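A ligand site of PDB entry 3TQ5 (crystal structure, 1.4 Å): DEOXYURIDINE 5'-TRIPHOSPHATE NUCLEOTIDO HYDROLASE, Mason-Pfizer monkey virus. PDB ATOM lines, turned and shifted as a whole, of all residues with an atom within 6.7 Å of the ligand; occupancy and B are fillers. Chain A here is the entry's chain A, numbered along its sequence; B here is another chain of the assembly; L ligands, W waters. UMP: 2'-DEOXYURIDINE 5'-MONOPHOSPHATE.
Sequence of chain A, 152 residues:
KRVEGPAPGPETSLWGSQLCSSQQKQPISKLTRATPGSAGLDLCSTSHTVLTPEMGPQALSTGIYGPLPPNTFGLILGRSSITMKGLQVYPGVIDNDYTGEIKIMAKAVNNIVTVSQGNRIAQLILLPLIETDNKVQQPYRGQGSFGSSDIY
Water W3 lies within hydrogen-bond range of an oxygen (OP3) of the ligand, the backbone NH of Val 93 and the backbone carbonyl oxygen of Gly 78 of chain B. Water W1 lies within hydrogen-bond range of O4 of the ligand, O of Tyr 90 and N of Met 105. Water W4 lies within hydrogen-bond range of an oxygen (OP1) of the ligand (2.9 Å), the backbone NH (N) of Ser 81 of chain B (3.1 Å) and the side-chain hydroxyl (OG) of Ser 80 of chain B (3.4 Å). Water W2 bridges an oxygen (OP1) of the ligand (3.0 Å) and the guanidinium group of Arg 79 of chain B (3.5 Å).
The backbone NH (N) of Lys 103 is in hydrogen-bond range of an oxygen (O2) of the ligand (2.9 Å). O of Lys 103 is in hydrogen-bond range of N3 of the ligand. The guanidinium group (NH2) of Arg 79 of chain B lies within salt-bridge range of an oxygen (OP1) of the ligand (2.7 Å). An oxygen (O3') of the ligand sits at hydrogen-bond distance from the backbone NH of Asp 95 (3.0 Å). The side-chain carboxylate of Asp 95 is in hydrogen-bond range of an oxygen (O3') of the ligand, 2.8 Å away. The backbone NH (N) of Ser 80 of chain B lies within hydrogen-bond range of an oxygen (OP3) of the ligand (2.8 Å). An oxygen (O5') of the ligand is in hydrogen-bond range of the side-chain hydroxyl of Ser 80 of chain B, at 2.9 Å. An oxygen (OP2) of the ligand sits close to the backbone carbonyl oxygen (O) of Val 93. OP3 of the ligand lies within hydrogen-bond range of NE2 of Gln 123 of chain B, 3.3 Å away.
The backbone NH (N) of Ala 39 of chain B sits at hydrogen-bond distance from the side-chain carboxylate (OD1) of Asp 95 (2.8 Å). The side-chain amide nitrogen (NE2) of Gln 123 of chain B is in hydrogen-bond range of the backbone carbonyl oxygen (O) of Gly 78 of chain B (2.9 Å). The backbone carbonyl oxygen (O) of Met 105 lies within hydrogen-bond range of the backbone NH (N) of Tyr 90, 2.9 Å away. The backbone carbonyl oxygen (O) of Gly 92 is in hydrogen-bond range of the backbone NH (N) of Ile 76, 2.8 Å away. The backbone carbonyl oxygen (O) of Glu 101 lies within hydrogen-bond range of the side-chain hydroxyl (OH) of Tyr 98, 2.5 Å away.
CG1 of Ile 76 touches O4 of the ligand (3.97 Å). CA of Gly 92 touches O4 of the ligand, at 3.4 Å. Ile 94 touches the ligand (CD1 to C2, 3.6 Å). CB of Tyr 98 touches O3' of the ligand, at 3.6 Å. Glu 101 touches the ligand (O to O2, 3.6 Å). CA of Ile 102 touches O2 of the ligand (3.5 Å). Met 105 touches the ligand. Gly 78 of chain B touches the ligand. 14 residues have an atom within 4 Å of the ligand: Ile 76, Gly 92, Val 93, Ile 94, Asp 95, Tyr 98, Glu 101, Ile 102, Lys 103, Met 105, Gly 78 of chain B, Arg 79 of chain B, Ser 80 of chain B and Gln 123 of chain B.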
ATOM      1  N   ILE A  76      -4.221  -2.186  -5.188  1.00  0.00           N
ATOM      2  CA  ILE A  76      -5.645  -1.985  -4.915  1.00  0.00           C
ATOM      3  C   ILE A  76      -6.095  -2.979  -3.885  1.00  0.00           C
ATOM      4  O   ILE A  76      -5.899  -4.142  -4.098  1.00  0.00           O
ATOM      5  CB  ILE A  76      -6.449  -2.235  -6.208  1.00  0.00           C
ATOM      6  CG1 ILE A  76      -5.821  -1.434  -7.343  1.00  0.00           C
ATOM      7  CG2 ILE A  76      -7.903  -1.830  -6.005  1.00  0.00           C
ATOM      8  CD1 ILE A  76      -5.800  -0.010  -7.015  1.00  0.00           C
ATOM      9  N   VAL A  89     -12.893  -7.267  -2.916  1.00  0.00           N
ATOM     10  CA  VAL A  89     -12.011  -6.636  -3.923  1.00  0.00           C
ATOM     11  C   VAL A  89     -10.762  -7.522  -4.005  1.00  0.00           C
ATOM     12  O   VAL A  89     -10.125  -7.825  -2.993  1.00  0.00           O
ATOM     13  CB  VAL A  89     -11.614  -5.201  -3.471  1.00  0.00           C
ATOM     14  CG1 VAL A  89     -10.442  -4.654  -4.329  1.00  0.00           C
ATOM     15  CG2 VAL A  89     -12.781  -4.282  -3.483  1.00  0.00           C
ATOM     16  N   TYR A  90     -10.450  -8.002  -5.210  1.00  0.00           N
ATOM     17  CA  TYR A  90      -9.276  -8.801  -5.420  1.00  0.00           C
ATOM     18  C   TYR A  90      -8.081  -7.871  -5.452  1.00  0.00           C
ATOM     19  O   TYR A  90      -8.128  -6.857  -6.202  1.00  0.00           O
ATOM     20  CB  TYR A  90      -9.326  -9.557  -6.759  1.00  0.00           C
ATOM     21  CG  TYR A  90     -10.473 -10.521  -6.854  1.00  0.00           C
ATOM     22  CD1 TYR A  90     -10.386 -11.720  -6.224  1.00  0.00           C
ATOM     23  CD2 TYR A  90     -11.646 -10.208  -7.549  1.00  0.00           C
ATOM     24  CE1 TYR A  90     -11.451 -12.618  -6.282  1.00  0.00           C
ATOM     25  CE2 TYR A  90     -12.743 -11.111  -7.611  1.00  0.00           C
ATOM     26  CZ  TYR A  90     -12.596 -12.329  -6.969  1.00  0.00           C
ATOM     27  OH  TYR A  90     -13.578 -13.299  -7.002  1.00  0.00           O
ATOM     28  N   PRO A  91      -7.043  -8.167  -4.692  1.00  0.00           N
ATOM     29  CA  PRO A  91      -5.876  -7.300  -4.669  1.00  0.00           C
ATOM     30  C   PRO A  91      -5.324  -7.187  -6.066  1.00  0.00           C
ATOM     31  O   PRO A  91      -5.185  -8.183  -6.791  1.00  0.00           O
ATOM     32  CB  PRO A  91      -4.899  -8.029  -3.752  1.00  0.00           C
ATOM     33  CG  PRO A  91      -5.793  -8.753  -2.870  1.00  0.00           C
ATOM     34  CD  PRO A  91      -6.924  -9.246  -3.689  1.00  0.00           C
ATOM     35  N   GLY A  92      -5.002  -5.973  -6.438  1.00  0.00           N
ATOM     36  CA  GLY A  92      -4.558  -5.729  -7.807  1.00  0.00           C
ATOM     37  C   GLY A  92      -3.276  -4.919  -7.790  1.00  0.00           C
ATOM     38  O   GLY A  92      -3.150  -3.972  -7.046  1.00  0.00           O
ATOM     39  N   VAL A  93      -2.335  -5.336  -8.635  1.00  0.00           N
ATOM     40  CA  VAL A  93      -1.057  -4.684  -8.734  1.00  0.00           C
ATOM     41  C   VAL A  93      -1.115  -3.629  -9.847  1.00  0.00           C
ATOM     42  O   VAL A  93      -1.446  -3.930 -10.974  1.00  0.00           O
ATOM     43  CB  VAL A  93       0.012  -5.718  -9.088  1.00  0.00           C
ATOM     44  CG1 VAL A  93       1.351  -5.071  -9.366  1.00  0.00           C
ATOM     45  CG2 VAL A  93       0.126  -6.741  -8.001  1.00  0.00           C
ATOM     46  N   ILE A  94      -0.762  -2.405  -9.499  1.00  0.00           N
ATOM     47  CA  ILE A  94      -0.743  -1.316 -10.484  1.00  0.00           C
ATOM     48  C   ILE A  94       0.744  -1.040 -10.832  1.00  0.00           C
ATOM     49  O   ILE A  94       1.518  -0.590  -9.987  1.00  0.00           O
ATOM     50  CB  ILE A  94      -1.376  -0.024  -9.932  1.00  0.00           C
ATOM     51  CG1 ILE A  94      -2.768  -0.247  -9.304  1.00  0.00           C
ATOM     52  CG2 ILE A  94      -1.427   1.035 -11.029  1.00  0.00           C
ATOM     53  CD1 ILE A  94      -3.827  -0.998 -10.269  1.00  0.00           C
ATOM     54  N   ASP A  95       1.144  -1.285 -12.060  1.00  0.00           N
ATOM     55  CA  ASP A  95       2.539  -1.074 -12.396  1.00  0.00           C
ATOM     56  C   ASP A  95       2.847   0.418 -12.414  1.00  0.00           C
ATOM     57  O   ASP A  95       1.963   1.255 -12.708  1.00  0.00           O
ATOM     58  CB  ASP A  95       2.770  -1.720 -13.734  1.00  0.00           C
ATOM     59  CG  ASP A  95       2.560  -3.248 -13.651  1.00  0.00           C
ATOM     60  OD1 ASP A  95       3.204  -3.898 -12.766  1.00  0.00           O
ATOM     61  OD2 ASP A  95       1.710  -3.814 -14.380  1.00  0.00           O
ATOM     62  N   ASN A  96       4.129   0.698 -12.198  1.00  0.00           N
ATOM     63  CA  ASN A  96       4.578   2.123 -12.127  1.00  0.00           C
ATOM     64  C   ASN A  96       4.235   2.903 -13.393  1.00  0.00           C
ATOM     65  O   ASN A  96       3.812   4.081 -13.335  1.00  0.00           O
ATOM     66  CB  ASN A  96       6.075   2.207 -11.877  1.00  0.00           C
ATOM     67  CG  ASN A  96       6.568   3.655 -11.862  1.00  0.00           C
ATOM     68  OD1 ASN A  96       7.066   4.165 -12.862  1.00  0.00           O
ATOM     69  ND2 ASN A  96       6.357   4.319 -10.763  1.00  0.00           N
ATOM     70  N   ASP A  97       4.395   2.255 -14.540  1.00  0.00           N
ATOM     71  CA  ASP A  97       4.271   2.956 -15.823  1.00  0.00           C
ATOM     72  C   ASP A  97       2.931   2.695 -16.516  1.00  0.00           C
ATOM     73  O   ASP A  97       2.747   3.051 -17.719  1.00  0.00           O
ATOM     74  CB  ASP A  97       5.414   2.543 -16.715  1.00  0.00           C
ATOM     75  CG  ASP A  97       5.541   0.995 -16.838  1.00  0.00           C
ATOM     76  OD1 ASP A  97       4.786   0.190 -16.198  1.00  0.00           O
ATOM     77  OD2 ASP A  97       6.428   0.617 -17.607  1.00  0.00           O
ATOM     78  N   TYR A  98       1.974   2.144 -15.746  1.00  0.00           N
ATOM     79  CA  TYR A  98       0.648   1.953 -16.381  1.00  0.00           C
ATOM     80  C   TYR A  98      -0.008   3.326 -16.596  1.00  0.00           C
ATOM     81  O   TYR A  98      -0.069   4.114 -15.639  1.00  0.00           O
ATOM     82  CB  TYR A  98      -0.244   1.219 -15.335  1.00  0.00           C
ATOM     83  CG  TYR A  98      -1.686   0.978 -15.759  1.00  0.00           C
ATOM     84  CD1 TYR A  98      -1.970   0.088 -16.796  1.00  0.00           C
ATOM     85  CD2 TYR A  98      -2.743   1.505 -15.031  1.00  0.00           C
ATOM     86  CE1 TYR A  98      -3.325  -0.163 -17.181  1.00  0.00           C
ATOM     87  CE2 TYR A  98      -4.069   1.222 -15.388  1.00  0.00           C
ATOM     88  CZ  TYR A  98      -4.343   0.383 -16.469  1.00  0.00           C
ATOM     89  OH  TYR A  98      -5.670   0.108 -16.789  1.00  0.00           O
ATOM     90  N   GLY A 100      -3.251   3.501 -18.223  1.00  0.00           N
ATOM     91  CA  GLY A 100      -4.659   3.263 -18.442  1.00  0.00           C
ATOM     92  C   GLY A 100      -5.481   3.602 -17.219  1.00  0.00           C
ATOM     93  O   GLY A 100      -4.995   4.142 -16.228  1.00  0.00           O
ATOM     94  N   GLU A 101      -6.764   3.233 -17.286  1.00  0.00           N
ATOM     95  CA  GLU A 101      -7.656   3.508 -16.177  1.00  0.00           C
ATOM     96  C   GLU A 101      -7.496   2.456 -15.095  1.00  0.00           C
ATOM     97  O   GLU A 101      -7.434   1.262 -15.405  1.00  0.00           O
ATOM     98  CB  GLU A 101      -9.110   3.457 -16.648  1.00  0.00           C
ATOM     99  CG  GLU A 101     -10.084   3.865 -15.593  1.00  0.00           C
ATOM    100  CD  GLU A 101     -11.543   3.733 -16.065  1.00  0.00           C
ATOM    101  OE1 GLU A 101     -11.743   3.282 -17.207  1.00  0.00           O
ATOM    102  OE2 GLU A 101     -12.446   4.065 -15.303  1.00  0.00           O
ATOM    103  N   ILE A 102      -7.405   2.915 -13.866  1.00  0.00           N
ATOM    104  CA  ILE A 102      -7.323   2.006 -12.700  1.00  0.00           C
ATOM    105  C   ILE A 102      -8.731   1.476 -12.426  1.00  0.00           C
ATOM    106  O   ILE A 102      -9.668   2.234 -12.277  1.00  0.00           O
ATOM    107  CB  ILE A 102      -6.743   2.781 -11.504  1.00  0.00           C
ATOM    108  CG1 ILE A 102      -5.270   3.089 -11.756  1.00  0.00           C
ATOM    109  CG2 ILE A 102      -6.815   1.900 -10.211  1.00  0.00           C
ATOM    110  CD1 ILE A 102      -4.572   4.009 -10.739  1.00  0.00           C
ATOM    111  N   LYS A 103      -8.909   0.181 -12.588  1.00  0.00           N
ATOM    112  CA  LYS A 103     -10.234  -0.395 -12.322  1.00  0.00           C
ATOM    113  C   LYS A 103     -10.149  -1.312 -11.079  1.00  0.00           C
ATOM    114  O   LYS A 103      -9.090  -1.854 -10.706  1.00  0.00           O
ATOM    115  CB  LYS A 103     -10.688  -1.202 -13.550  1.00  0.00           C
ATOM    116  CG  LYS A 103     -10.933  -0.277 -14.755  1.00  0.00           C
ATOM    117  CD  LYS A 103     -11.820  -0.942 -15.777  1.00  0.00           C
ATOM    118  CE  LYS A 103     -11.926  -0.143 -17.063  1.00  0.00           C
ATOM    119  NZ  LYS A 103     -12.658  -1.001 -18.064  1.00  0.00           N
ATOM    120  N   ILE A 104     -11.288  -1.479 -10.429  1.00  0.00           N
ATOM    121  CA  ILE A 104     -11.367  -2.242  -9.211  1.00  0.00           C
ATOM    122  C   ILE A 104     -11.940  -3.611  -9.621  1.00  0.00           C
ATOM    123  O   ILE A 104     -12.964  -3.660 -10.291  1.00  0.00           O
ATOM    124  CB  ILE A 104     -12.322  -1.596  -8.217  1.00  0.00           C
ATOM    125  CG1 ILE A 104     -11.806  -0.198  -7.811  1.00  0.00           C
ATOM    126  CG2 ILE A 104     -12.512  -2.404  -6.902  1.00  0.00           C
ATOM    127  CD1 ILE A 104     -12.836   0.729  -7.198  1.00  0.00           C
ATOM    128  N   MET A 105     -11.234  -4.684  -9.277  1.00  0.00           N
ATOM    129  CA  MET A 105     -11.744  -6.062  -9.594  1.00  0.00           C
ATOM    130  C   MET A 105     -12.542  -6.517  -8.375  1.00  0.00           C
ATOM    131  O   MET A 105     -11.966  -6.588  -7.304  1.00  0.00           O
ATOM    132  CB  MET A 105     -10.583  -7.034  -9.817  1.00  0.00           C
ATOM    133  CG  MET A 105      -9.721  -6.552 -11.012  1.00  0.00           C
ATOM    134  SD  MET A 105      -8.484  -7.734 -11.453  1.00  0.00           S
ATOM    135  CE  MET A 105      -7.420  -7.660  -9.967  1.00  0.00           C
ATOM    136  N   ALA B  39       5.792  -4.213 -11.659  1.00  0.00           N
ATOM    137  CA  ALA B  39       6.074  -4.373 -10.261  1.00  0.00           C
ATOM    138  C   ALA B  39       6.443  -5.811  -9.986  1.00  0.00           C
ATOM    139  O   ALA B  39       7.202  -6.070  -9.063  1.00  0.00           O
ATOM    140  CB  ALA B  39       4.868  -3.985  -9.479  1.00  0.00           C
ATOM    141  N   GLY B  40       5.872  -6.758 -10.726  1.00  0.00           N
ATOM    142  CA  GLY B  40       5.999  -8.176 -10.349  1.00  0.00           C
ATOM    143  C   GLY B  40       6.860  -8.966 -11.290  1.00  0.00           C
ATOM    144  O   GLY B  40       7.047  -8.568 -12.452  1.00  0.00           O
ATOM    145  N   GLY B  78      -2.143 -12.167  -7.779  1.00  0.00           N
ATOM    146  CA  GLY B  78      -2.661 -12.518  -9.113  1.00  0.00           C
ATOM    147  C   GLY B  78      -2.269 -11.546 -10.209  1.00  0.00           C
ATOM    148  O   GLY B  78      -1.830 -10.415  -9.974  1.00  0.00           O
ATOM    149  N   ARG B  79      -2.393 -12.045 -11.446  1.00  0.00           N
ATOM    150  CA  ARG B  79      -2.383 -11.149 -12.594  1.00  0.00           C
ATOM    151  C   ARG B  79      -3.785 -10.727 -12.863  1.00  0.00           C
ATOM    152  O   ARG B  79      -4.683 -11.596 -12.868  1.00  0.00           O
ATOM    153  CB  ARG B  79      -1.850 -11.897 -13.849  1.00  0.00           C
ATOM    154  CG  ARG B  79      -0.341 -12.111 -13.870  1.00  0.00           C
ATOM    155  CD  ARG B  79       0.259 -10.837 -14.504  1.00  0.00           C
ATOM    156  NE  ARG B  79       1.714 -10.764 -14.317  1.00  0.00           N
ATOM    157  CZ  ARG B  79       2.421  -9.658 -14.303  1.00  0.00           C
ATOM    158  NH1 ARG B  79       3.744  -9.746 -14.133  1.00  0.00           N
ATOM    159  NH2 ARG B  79       1.840  -8.490 -14.558  1.00  0.00           N
ATOM    160  N   SER B  80      -4.079  -9.453 -13.195  1.00  0.00           N
ATOM    161  CA  SER B  80      -5.459  -9.060 -13.342  1.00  0.00           C
ATOM    162  C   SER B  80      -6.136  -9.757 -14.506  1.00  0.00           C
ATOM    163  O   SER B  80      -7.347 -10.061 -14.415  1.00  0.00           O
ATOM    164  CB  SER B  80      -5.563  -7.525 -13.547  1.00  0.00           C
ATOM    165  OG  SER B  80      -4.859  -7.111 -14.703  1.00  0.00           O
ATOM    166  N   SER B  81      -5.373 -10.070 -15.577  1.00  0.00           N
ATOM    167  CA  SER B  81      -6.010 -10.722 -16.732  1.00  0.00           C
ATOM    168  C   SER B  81      -6.569 -12.093 -16.353  1.00  0.00           C
ATOM    169  O   SER B  81      -7.600 -12.511 -16.932  1.00  0.00           O
ATOM    170  CB  SER B  81      -5.071 -10.790 -17.944  1.00  0.00           C
ATOM    171  OG  SER B  81      -3.934 -11.528 -17.588  1.00  0.00           O
ATOM    172  N   GLN B 123       2.223 -13.363 -10.011  1.00  0.00           N
ATOM    173  CA  GLN B 123       3.415 -12.556 -10.026  1.00  0.00           C
ATOM    174  C   GLN B 123       3.983 -12.474  -8.620  1.00  0.00           C
ATOM    175  O   GLN B 123       3.222 -12.476  -7.645  1.00  0.00           O
ATOM    176  CB  GLN B 123       3.139 -11.136 -10.607  1.00  0.00           C
ATOM    177  CG  GLN B 123       2.058 -10.332  -9.855  1.00  0.00           C
ATOM    178  CD  GLN B 123       1.761  -9.079 -10.626  1.00  0.00           C
ATOM    179  OE1 GLN B 123       2.668  -8.303 -10.914  1.00  0.00           O
ATOM    180  NE2 GLN B 123       0.489  -8.892 -10.973  1.00  0.00           N
HETATM  181  N1  UMP L   1      -4.932  -3.081 -13.087  1.00  0.00           N
HETATM  182  C2  UMP L   1      -6.049  -2.427 -12.647  1.00  0.00           C
HETATM  183  N3  UMP L   1      -6.721  -2.861 -11.525  1.00  0.00           N
HETATM  184  C4  UMP L   1      -6.273  -3.991 -10.838  1.00  0.00           C
HETATM  185  C5  UMP L   1      -5.135  -4.673 -11.285  1.00  0.00           C
HETATM  186  C6  UMP L   1      -4.439  -4.205 -12.401  1.00  0.00           C
HETATM  187  O2  UMP L   1      -6.539  -1.398 -13.191  1.00  0.00           O
HETATM  188  O4  UMP L   1      -6.912  -4.314  -9.844  1.00  0.00           O
HETATM  189  C1' UMP L   1      -4.242  -2.547 -14.283  1.00  0.00           C
HETATM  190  C2' UMP L   1      -2.939  -1.895 -13.728  1.00  0.00           C
HETATM  191  C3' UMP L   1      -1.820  -2.912 -14.017  1.00  0.00           C
HETATM  192  C4' UMP L   1      -2.395  -3.597 -15.247  1.00  0.00           C
HETATM  193  O3' UMP L   1      -0.581  -2.249 -14.277  1.00  0.00           O
HETATM  194  O4' UMP L   1      -3.802  -3.616 -15.101  1.00  0.00           O
HETATM  195  C5' UMP L   1      -1.858  -4.995 -15.492  1.00  0.00           C
HETATM  196  O5' UMP L   1      -2.293  -5.739 -14.350  1.00  0.00           O
HETATM  197  P   UMP L   1      -1.279  -6.834 -13.722  1.00  0.00           P
HETATM  198  OP1 UMP L   1      -0.685  -7.551 -14.759  1.00  0.00           O
HETATM  199  OP2 UMP L   1      -0.214  -5.948 -12.893  1.00  0.00           O
HETATM  200  OP3 UMP L   1      -2.042  -7.555 -12.695  1.00  0.00           O
HETATM  201  O   HOH W   1      -8.757  -4.701  -7.826  1.00  0.00           O
HETATM  202  O   HOH W   2       0.380  -7.352 -17.503  1.00  0.00           O
HETATM  203  O   HOH W   3      -3.086  -7.554 -10.208  1.00  0.00           O
HETATM  204  O   HOH W   4      -2.546  -9.129 -16.272  1.00  0.00           O
